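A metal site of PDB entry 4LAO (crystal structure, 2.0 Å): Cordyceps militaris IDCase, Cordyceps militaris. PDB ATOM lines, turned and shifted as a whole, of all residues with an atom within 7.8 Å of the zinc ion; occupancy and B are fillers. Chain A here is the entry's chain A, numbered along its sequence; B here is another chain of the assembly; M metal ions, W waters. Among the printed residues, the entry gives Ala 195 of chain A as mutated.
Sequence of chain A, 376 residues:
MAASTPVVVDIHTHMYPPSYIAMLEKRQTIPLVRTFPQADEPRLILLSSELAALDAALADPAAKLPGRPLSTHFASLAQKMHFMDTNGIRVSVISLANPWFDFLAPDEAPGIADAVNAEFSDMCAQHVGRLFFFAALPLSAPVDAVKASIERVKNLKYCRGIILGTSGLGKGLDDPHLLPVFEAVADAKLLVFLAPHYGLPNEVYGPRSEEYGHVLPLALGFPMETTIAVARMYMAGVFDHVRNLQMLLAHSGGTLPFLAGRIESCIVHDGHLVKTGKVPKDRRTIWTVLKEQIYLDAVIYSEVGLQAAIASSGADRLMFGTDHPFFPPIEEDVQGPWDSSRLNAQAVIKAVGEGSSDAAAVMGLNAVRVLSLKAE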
ATOM      1  N   HIS A  12     -22.180  19.888  -4.502  1.00  0.00           N
ATOM      2  CA  HIS A  12     -21.931  20.104  -5.920  1.00  0.00           C
ATOM      3  C   HIS A  12     -20.915  21.233  -6.070  1.00  0.00           C
ATOM      4  O   HIS A  12     -21.281  22.411  -6.190  1.00  0.00           O
ATOM      5  CB  HIS A  12     -23.227  20.447  -6.657  1.00  0.00           C
ATOM      6  CG  HIS A  12     -23.117  20.367  -8.145  1.00  0.00           C
ATOM      7  ND1 HIS A  12     -24.200  20.126  -8.966  1.00  0.00           N
ATOM      8  CD2 HIS A  12     -22.053  20.497  -8.976  1.00  0.00           C
ATOM      9  CE1 HIS A  12     -23.815  20.104 -10.225  1.00  0.00           C
ATOM     10  NE2 HIS A  12     -22.504  20.321 -10.259  1.00  0.00           N
ATOM     11  N   THR A  13     -19.637  20.868  -6.044  1.00  0.00           N
ATOM     12  CA  THR A  13     -18.551  21.829  -6.027  1.00  0.00           C
ATOM     13  C   THR A  13     -17.275  21.167  -6.569  1.00  0.00           C
ATOM     14  O   THR A  13     -16.931  20.054  -6.169  1.00  0.00           O
ATOM     15  CB  THR A  13     -18.357  22.440  -4.613  1.00  0.00           C
ATOM     16  OG1 THR A  13     -17.172  23.238  -4.567  1.00  0.00           O
ATOM     17  CG2 THR A  13     -18.282  21.351  -3.531  1.00  0.00           C
ATOM     18  N   HIS A  14     -16.616  21.834  -7.515  1.00  0.00           N
ATOM     19  CA  HIS A  14     -15.577  21.187  -8.325  1.00  0.00           C
ATOM     20  C   HIS A  14     -14.172  21.775  -8.153  1.00  0.00           C
ATOM     21  O   HIS A  14     -14.010  22.918  -7.732  1.00  0.00           O
ATOM     22  CB  HIS A  14     -15.943  21.250  -9.809  1.00  0.00           C
ATOM     23  CG  HIS A  14     -17.307  20.730 -10.127  1.00  0.00           C
ATOM     24  ND1 HIS A  14     -17.658  19.404  -9.979  1.00  0.00           N
ATOM     25  CD2 HIS A  14     -18.410  21.361 -10.608  1.00  0.00           C
ATOM     26  CE1 HIS A  14     -18.919  19.238 -10.337  1.00  0.00           C
ATOM     27  NE2 HIS A  14     -19.398  20.408 -10.730  1.00  0.00           N
ATOM     28  N   SER A  95     -15.585  17.432  -6.074  1.00  0.00           N
ATOM     29  CA  SER A  95     -15.459  16.427  -7.123  1.00  0.00           C
ATOM     30  C   SER A  95     -14.647  16.987  -8.280  1.00  0.00           C
ATOM     31  O   SER A  95     -14.653  18.190  -8.523  1.00  0.00           O
ATOM     32  CB  SER A  95     -16.843  15.972  -7.598  1.00  0.00           C
ATOM     33  OG  SER A  95     -17.633  17.077  -8.019  1.00  0.00           O
ATOM     34  N   LEU A  96     -13.940  16.107  -8.980  1.00  0.00           N
ATOM     35  CA  LEU A  96     -13.253  16.481 -10.196  1.00  0.00           C
ATOM     36  C   LEU A  96     -14.268  17.004 -11.207  1.00  0.00           C
ATOM     37  O   LEU A  96     -15.381  16.466 -11.307  1.00  0.00           O
ATOM     38  CB  LEU A  96     -12.487  15.275 -10.767  1.00  0.00           C
ATOM     39  CG  LEU A  96     -11.570  15.466 -11.978  1.00  0.00           C
ATOM     40  CD1 LEU A  96     -10.428  16.429 -11.687  1.00  0.00           C
ATOM     41  CD2 LEU A  96     -11.030  14.113 -12.433  1.00  0.00           C
ATOM     42  N   ALA A  97     -13.911  18.061 -11.917  1.00  0.00           N
ATOM     43  CA  ALA A  97     -14.802  18.634 -12.921  1.00  0.00           C
ATOM     44  C   ALA A  97     -14.648  17.894 -14.251  1.00  0.00           C
ATOM     45  O   ALA A  97     -13.656  17.201 -14.476  1.00  0.00           O
ATOM     46  CB  ALA A  97     -14.532  20.116 -13.094  1.00  0.00           C
ATOM     47  N   ASN A  98     -15.643  18.056 -15.119  1.00  0.00           N
ATOM     48  CA  ASN A  98     -15.547  17.603 -16.509  1.00  0.00           C
ATOM     49  C   ASN A  98     -14.241  18.118 -17.137  1.00  0.00           C
ATOM     50  O   ASN A  98     -13.826  19.230 -16.839  1.00  0.00           O
ATOM     51  CB  ASN A  98     -16.769  18.079 -17.308  1.00  0.00           C
ATOM     52  CG  ASN A  98     -16.846  19.599 -17.408  1.00  0.00           C
ATOM     53  OD1 ASN A  98     -17.035  20.291 -16.406  1.00  0.00           O
ATOM     54  ND2 ASN A  98     -16.711  20.117 -18.625  1.00  0.00           N
ATOM     55  N   TRP A 100     -13.146  14.935 -16.562  1.00  0.00           N
ATOM     56  CA  TRP A 100     -12.721  13.808 -15.722  1.00  0.00           C
ATOM     57  C   TRP A 100     -11.592  12.997 -16.357  1.00  0.00           C
ATOM     58  O   TRP A 100     -10.578  13.562 -16.775  1.00  0.00           O
ATOM     59  CB  TRP A 100     -13.931  12.933 -15.341  1.00  0.00           C
ATOM     60  CG  TRP A 100     -15.080  13.733 -14.810  1.00  0.00           C
ATOM     61  CD1 TRP A 100     -15.175  14.311 -13.582  1.00  0.00           C
ATOM     62  CD2 TRP A 100     -16.301  14.053 -15.495  1.00  0.00           C
ATOM     63  NE1 TRP A 100     -16.372  14.967 -13.451  1.00  0.00           N
ATOM     64  CE2 TRP A 100     -17.086  14.824 -14.614  1.00  0.00           C
ATOM     65  CE3 TRP A 100     -16.810  13.751 -16.763  1.00  0.00           C
ATOM     66  CZ2 TRP A 100     -18.354  15.308 -14.959  1.00  0.00           C
ATOM     67  CZ3 TRP A 100     -18.079  14.234 -17.108  1.00  0.00           C
ATOM     68  CH2 TRP A 100     -18.827  15.001 -16.205  1.00  0.00           C
ATOM     69  N   ILE A 163     -18.074  10.329  -8.766  1.00  0.00           N
ATOM     70  CA  ILE A 163     -18.644  11.210  -9.788  1.00  0.00           C
ATOM     71  C   ILE A 163     -18.557  10.507 -11.145  1.00  0.00           C
ATOM     72  O   ILE A 163     -17.509   9.984 -11.517  1.00  0.00           O
ATOM     73  CB  ILE A 163     -18.018  12.633  -9.820  1.00  0.00           C
ATOM     74  CG1 ILE A 163     -18.700  13.487 -10.904  1.00  0.00           C
ATOM     75  CG2 ILE A 163     -16.508  12.592  -9.987  1.00  0.00           C
ATOM     76  CD1 ILE A 163     -18.554  14.992 -10.720  1.00  0.00           C
ATOM     77  N   PHE A 193     -22.672  10.326  -7.977  1.00  0.00           N
ATOM     78  CA  PHE A 193     -23.015  11.670  -8.406  1.00  0.00           C
ATOM     79  C   PHE A 193     -22.937  11.724  -9.925  1.00  0.00           C
ATOM     80  O   PHE A 193     -21.855  11.669 -10.502  1.00  0.00           O
ATOM     81  CB  PHE A 193     -22.065  12.691  -7.743  1.00  0.00           C
ATOM     82  CG  PHE A 193     -22.324  14.127  -8.119  1.00  0.00           C
ATOM     83  CD1 PHE A 193     -23.617  14.584  -8.369  1.00  0.00           C
ATOM     84  CD2 PHE A 193     -21.281  15.041  -8.165  1.00  0.00           C
ATOM     85  CE1 PHE A 193     -23.849  15.916  -8.699  1.00  0.00           C
ATOM     86  CE2 PHE A 193     -21.504  16.370  -8.492  1.00  0.00           C
ATOM     87  CZ  PHE A 193     -22.799  16.809  -8.757  1.00  0.00           C
ATOM     88  N   LEU A 194     -24.095  11.813 -10.571  1.00  0.00           N
ATOM     89  CA  LEU A 194     -24.157  11.891 -12.028  1.00  0.00           C
ATOM     90  C   LEU A 194     -24.126  13.340 -12.486  1.00  0.00           C
ATOM     91  O   LEU A 194     -24.934  14.164 -12.052  1.00  0.00           O
ATOM     92  CB  LEU A 194     -25.411  11.192 -12.571  1.00  0.00           C
ATOM     93  CG  LEU A 194     -25.574  11.240 -14.097  1.00  0.00           C
ATOM     94  CD1 LEU A 194     -24.425  10.517 -14.808  1.00  0.00           C
ATOM     95  CD2 LEU A 194     -26.903  10.640 -14.522  1.00  0.00           C
ATOM     96  N   ALA A 195     -23.195  13.640 -13.378  1.00  0.00           N
ATOM     97  CA  ALA A 195     -22.964  15.002 -13.837  1.00  0.00           C
ATOM     98  C   ALA A 195     -22.904  15.062 -15.362  1.00  0.00           C
ATOM     99  O   ALA A 195     -22.392  14.146 -15.994  1.00  0.00           O
ATOM    100  CB  ALA A 195     -21.688  15.562 -13.233  1.00  0.00           C
ATOM    101  N   PRO A 196     -23.434  16.155 -15.944  1.00  0.00           N
ATOM    102  CA  PRO A 196     -23.404  16.345 -17.395  1.00  0.00           C
ATOM    103  C   PRO A 196     -22.079  16.935 -17.877  1.00  0.00           C
ATOM    104  O   PRO A 196     -21.299  17.433 -17.064  1.00  0.00           O
ATOM    105  CB  PRO A 196     -24.534  17.348 -17.625  1.00  0.00           C
ATOM    106  CG  PRO A 196     -24.527  18.186 -16.397  1.00  0.00           C
ATOM    107  CD  PRO A 196     -24.132  17.263 -15.270  1.00  0.00           C
ATOM    108  N   PHE A 222     -26.965  20.878 -20.685  1.00  0.00           N
ATOM    109  CA  PHE A 222     -26.552  20.101 -19.518  1.00  0.00           C
ATOM    110  C   PHE A 222     -27.710  19.394 -18.797  1.00  0.00           C
ATOM    111  O   PHE A 222     -27.652  18.177 -18.603  1.00  0.00           O
ATOM    112  CB  PHE A 222     -25.742  20.952 -18.524  1.00  0.00           C
ATOM    113  CG  PHE A 222     -24.288  21.110 -18.870  1.00  0.00           C
ATOM    114  CD1 PHE A 222     -23.721  20.413 -19.939  1.00  0.00           C
ATOM    115  CD2 PHE A 222     -23.471  21.944 -18.120  1.00  0.00           C
ATOM    116  CE1 PHE A 222     -22.379  20.561 -20.250  1.00  0.00           C
ATOM    117  CE2 PHE A 222     -22.123  22.088 -18.419  1.00  0.00           C
ATOM    118  CZ  PHE A 222     -21.577  21.396 -19.484  1.00  0.00           C
ATOM    119  N   ALA A 250     -27.311  15.799 -10.777  1.00  0.00           N
ATOM    120  CA  ALA A 250     -26.936  17.201 -10.916  1.00  0.00           C
ATOM    121  C   ALA A 250     -28.133  18.055 -11.329  1.00  0.00           C
ATOM    122  O   ALA A 250     -29.009  17.588 -12.074  1.00  0.00           O
ATOM    123  CB  ALA A 250     -25.807  17.354 -11.914  1.00  0.00           C
ATOM    124  N   HIS A 251     -28.151  19.297 -10.846  1.00  0.00           N
ATOM    125  CA  HIS A 251     -29.163  20.295 -11.230  1.00  0.00           C
ATOM    126  C   HIS A 251     -30.605  19.806 -11.069  1.00  0.00           C
ATOM    127  O   HIS A 251     -31.435  19.941 -11.971  1.00  0.00           O
ATOM    128  CB  HIS A 251     -28.895  20.815 -12.647  1.00  0.00           C
ATOM    129  CG  HIS A 251     -27.451  21.048 -12.943  1.00  0.00           C
ATOM    130  ND1 HIS A 251     -26.796  20.429 -13.992  1.00  0.00           N
ATOM    131  CD2 HIS A 251     -26.521  21.819 -12.325  1.00  0.00           C
ATOM    132  CE1 HIS A 251     -25.531  20.814 -14.005  1.00  0.00           C
ATOM    133  NE2 HIS A 251     -25.337  21.664 -13.001  1.00  0.00           N
ATOM    134  N   ASP A 297     -29.791  17.237  -6.256  1.00  0.00           N
ATOM    135  CA  ASP A 297     -29.199  18.453  -5.713  1.00  0.00           C
ATOM    136  C   ASP A 297     -30.226  19.583  -5.837  1.00  0.00           C
ATOM    137  O   ASP A 297     -31.236  19.438  -6.523  1.00  0.00           O
ATOM    138  CB  ASP A 297     -27.823  18.781  -6.315  1.00  0.00           C
ATOM    139  CG  ASP A 297     -27.872  19.433  -7.689  1.00  0.00           C
ATOM    140  OD1 ASP A 297     -28.910  20.003  -8.083  1.00  0.00           O
ATOM    141  OD2 ASP A 297     -26.840  19.390  -8.387  1.00  0.00           O
ATOM    142  N   VAL A 299     -29.560  22.632  -7.010  1.00  0.00           N
ATOM    143  CA  VAL A 299     -28.992  23.635  -7.913  1.00  0.00           C
ATOM    144  C   VAL A 299     -29.978  23.917  -9.058  1.00  0.00           C
ATOM    145  O   VAL A 299     -29.813  23.417 -10.166  1.00  0.00           O
ATOM    146  CB  VAL A 299     -27.601  23.207  -8.456  1.00  0.00           C
ATOM    147  CG1 VAL A 299     -26.938  24.350  -9.211  1.00  0.00           C
ATOM    148  CG2 VAL A 299     -26.705  22.759  -7.313  1.00  0.00           C
ATOM    149  N   THR A 322     -23.680  24.359  -5.034  1.00  0.00           N
ATOM    150  CA  THR A 322     -23.395  25.683  -5.620  1.00  0.00           C
ATOM    151  C   THR A 322     -22.889  25.641  -7.066  1.00  0.00           C
ATOM    152  O   THR A 322     -22.967  26.647  -7.768  1.00  0.00           O
ATOM    153  CB  THR A 322     -22.354  26.467  -4.793  1.00  0.00           C
ATOM    154  OG1 THR A 322     -21.111  25.757  -4.800  1.00  0.00           O
ATOM    155  CG2 THR A 322     -22.833  26.674  -3.355  1.00  0.00           C
ATOM    156  N   ASP A 323     -22.374  24.490  -7.488  1.00  0.00           N
ATOM    157  CA  ASP A 323     -21.674  24.353  -8.768  1.00  0.00           C
ATOM    158  C   ASP A 323     -20.445  25.274  -8.880  1.00  0.00           C
ATOM    159  O   ASP A 323     -20.048  25.668  -9.976  1.00  0.00           O
ATOM    160  CB  ASP A 323     -22.634  24.543  -9.961  1.00  0.00           C
ATOM    161  CG  ASP A 323     -22.348  23.581 -11.100  1.00  0.00           C
ATOM    162  OD1 ASP A 323     -21.231  23.027 -11.167  1.00  0.00           O
ATOM    163  OD2 ASP A 323     -23.242  23.389 -11.947  1.00  0.00           O
ATOM    164  N   HIS A 324     -19.860  25.606  -7.731  1.00  0.00           N
ATOM    165  CA  HIS A 324     -18.584  26.331  -7.666  1.00  0.00           C
ATOM    166  C   HIS A 324     -17.531  25.533  -8.441  1.00  0.00           C
ATOM    167  O   HIS A 324     -17.446  24.314  -8.270  1.00  0.00           O
ATOM    168  CB  HIS A 324     -18.155  26.523  -6.206  1.00  0.00           C
ATOM    169  CG  HIS A 324     -16.921  27.341  -6.034  1.00  0.00           C
ATOM    170  ND1 HIS A 324     -15.685  26.783  -5.786  1.00  0.00           N
ATOM    171  CD2 HIS A 324     -16.720  28.679  -6.060  1.00  0.00           C
ATOM    172  CE1 HIS A 324     -14.778  27.740  -5.680  1.00  0.00           C
ATOM    173  NE2 HIS A 324     -15.381  28.907  -5.827  1.00  0.00           N
ATOM    174  N   PRO A 325     -16.715  26.212  -9.269  1.00  0.00           N
ATOM    175  CA  PRO A 325     -16.614  27.646  -9.484  1.00  0.00           C
ATOM    176  C   PRO A 325     -17.194  28.119 -10.827  1.00  0.00           C
ATOM    177  O   PRO A 325     -16.694  29.101 -11.394  1.00  0.00           O
ATOM    178  CB  PRO A 325     -15.092  27.853  -9.502  1.00  0.00           C
ATOM    179  CG  PRO A 325     -14.573  26.590 -10.121  1.00  0.00           C
ATOM    180  CD  PRO A 325     -15.612  25.505  -9.950  1.00  0.00           C
ATOM    181  N   PHE A 326     -18.224  27.450 -11.313  1.00  0.00           N
ATOM    182  CA  PHE A 326     -18.697  27.674 -12.680  1.00  0.00           C
ATOM    183  C   PHE A 326     -19.463  28.962 -12.959  1.00  0.00           C
ATOM    184  O   PHE A 326     -19.501  29.415 -14.105  1.00  0.00           O
ATOM    185  CB  PHE A 326     -19.470  26.452 -13.209  1.00  0.00           C
ATOM    186  CG  PHE A 326     -18.573  25.363 -13.708  1.00  0.00           C
ATOM    187  CD1 PHE A 326     -17.912  25.509 -14.925  1.00  0.00           C
ATOM    188  CD2 PHE A 326     -18.381  24.209 -12.970  1.00  0.00           C
ATOM    189  CE1 PHE A 326     -17.067  24.513 -15.395  1.00  0.00           C
ATOM    190  CE2 PHE A 326     -17.540  23.203 -13.443  1.00  0.00           C
ATOM    191  CZ  PHE A 326     -16.890  23.351 -14.653  1.00  0.00           C
ATOM    192  N   PHE A 327     -20.065  29.552 -11.939  1.00  0.00           N
ATOM    193  CA  PHE A 327     -20.835  30.781 -12.153  1.00  0.00           C
ATOM    194  C   PHE A 327     -20.385  31.938 -11.252  1.00  0.00           C
ATOM    195  O   PHE A 327     -21.151  32.377 -10.384  1.00  0.00           O
ATOM    196  CB  PHE A 327     -22.344  30.503 -12.035  1.00  0.00           C
ATOM    197  CG  PHE A 327     -22.843  29.503 -13.035  1.00  0.00           C
ATOM    198  CD1 PHE A 327     -23.155  29.892 -14.345  1.00  0.00           C
ATOM    199  CD2 PHE A 327     -23.001  28.169 -12.686  1.00  0.00           C
ATOM    200  CE1 PHE A 327     -23.616  28.968 -15.268  1.00  0.00           C
ATOM    201  CE2 PHE A 327     -23.465  27.235 -13.611  1.00  0.00           C
ATOM    202  CZ  PHE A 327     -23.765  27.639 -14.904  1.00  0.00           C
ATOM    203  N   ARG B 262     -32.875  28.493 -14.059  1.00  0.00           N
ATOM    204  CA  ARG B 262     -31.537  28.205 -14.587  1.00  0.00           C
ATOM    205  C   ARG B 262     -31.190  29.097 -15.783  1.00  0.00           C
ATOM    206  O   ARG B 262     -30.077  29.608 -15.879  1.00  0.00           O
ATOM    207  CB  ARG B 262     -31.391  26.729 -14.958  1.00  0.00           C
ATOM    208  CG  ARG B 262     -30.003  26.372 -15.480  1.00  0.00           C
ATOM    209  CD  ARG B 262     -29.846  24.902 -15.845  1.00  0.00           C
ATOM    210  NE  ARG B 262     -28.466  24.631 -16.229  1.00  0.00           N
ATOM    211  CZ  ARG B 262     -27.468  24.406 -15.370  1.00  0.00           C
ATOM    212  NH1 ARG B 262     -27.690  24.401 -14.060  1.00  0.00           N
ATOM    213  NH2 ARG B 262     -26.240  24.174 -15.829  1.00  0.00           N
HETATM  214 ZN    ZN M   1     -21.215  20.987 -11.699  1.00  0.00          ZN
HETATM  215  O   HOH W   1     -22.106  20.325 -13.628  1.00  0.00           O
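A ring nitrogen (ND1) of His 12 sits at hydrogen-bond distance from the side-chain carboxylate of Asp 297, 2.8 Å away.
The side-chain hydroxyl (OG) of Ser 95 sits at hydrogen-bond distance from a ring nitrogen (ND1) of His 14, at 3.0 Å.
The side-chain carboxylate (OD2) of Asp 323 is in hydrogen-bond range of a ring nitrogen (NE2) of His 251 (2.9 Å).
The backbone NH (N) of Thr 322 is in hydrogen-bond range of the backbone carbonyl oxygen (O) of His 12.
O of His 324 lies within hydrogen-bond range of N of His 14 (2.7 Å).
The zinc ion is bound by a ring nitrogen (NE2) of His 12 (2.0 Å), the side-chain carboxylate (OD1) of Asp 323 (2.1 Å), a ring nitrogen (NE2) of His 14 (2.1 Å) and water W1 (2.2 Å).
Of the 25 residues printed, 3 come within 4 Å of the zinc ion.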
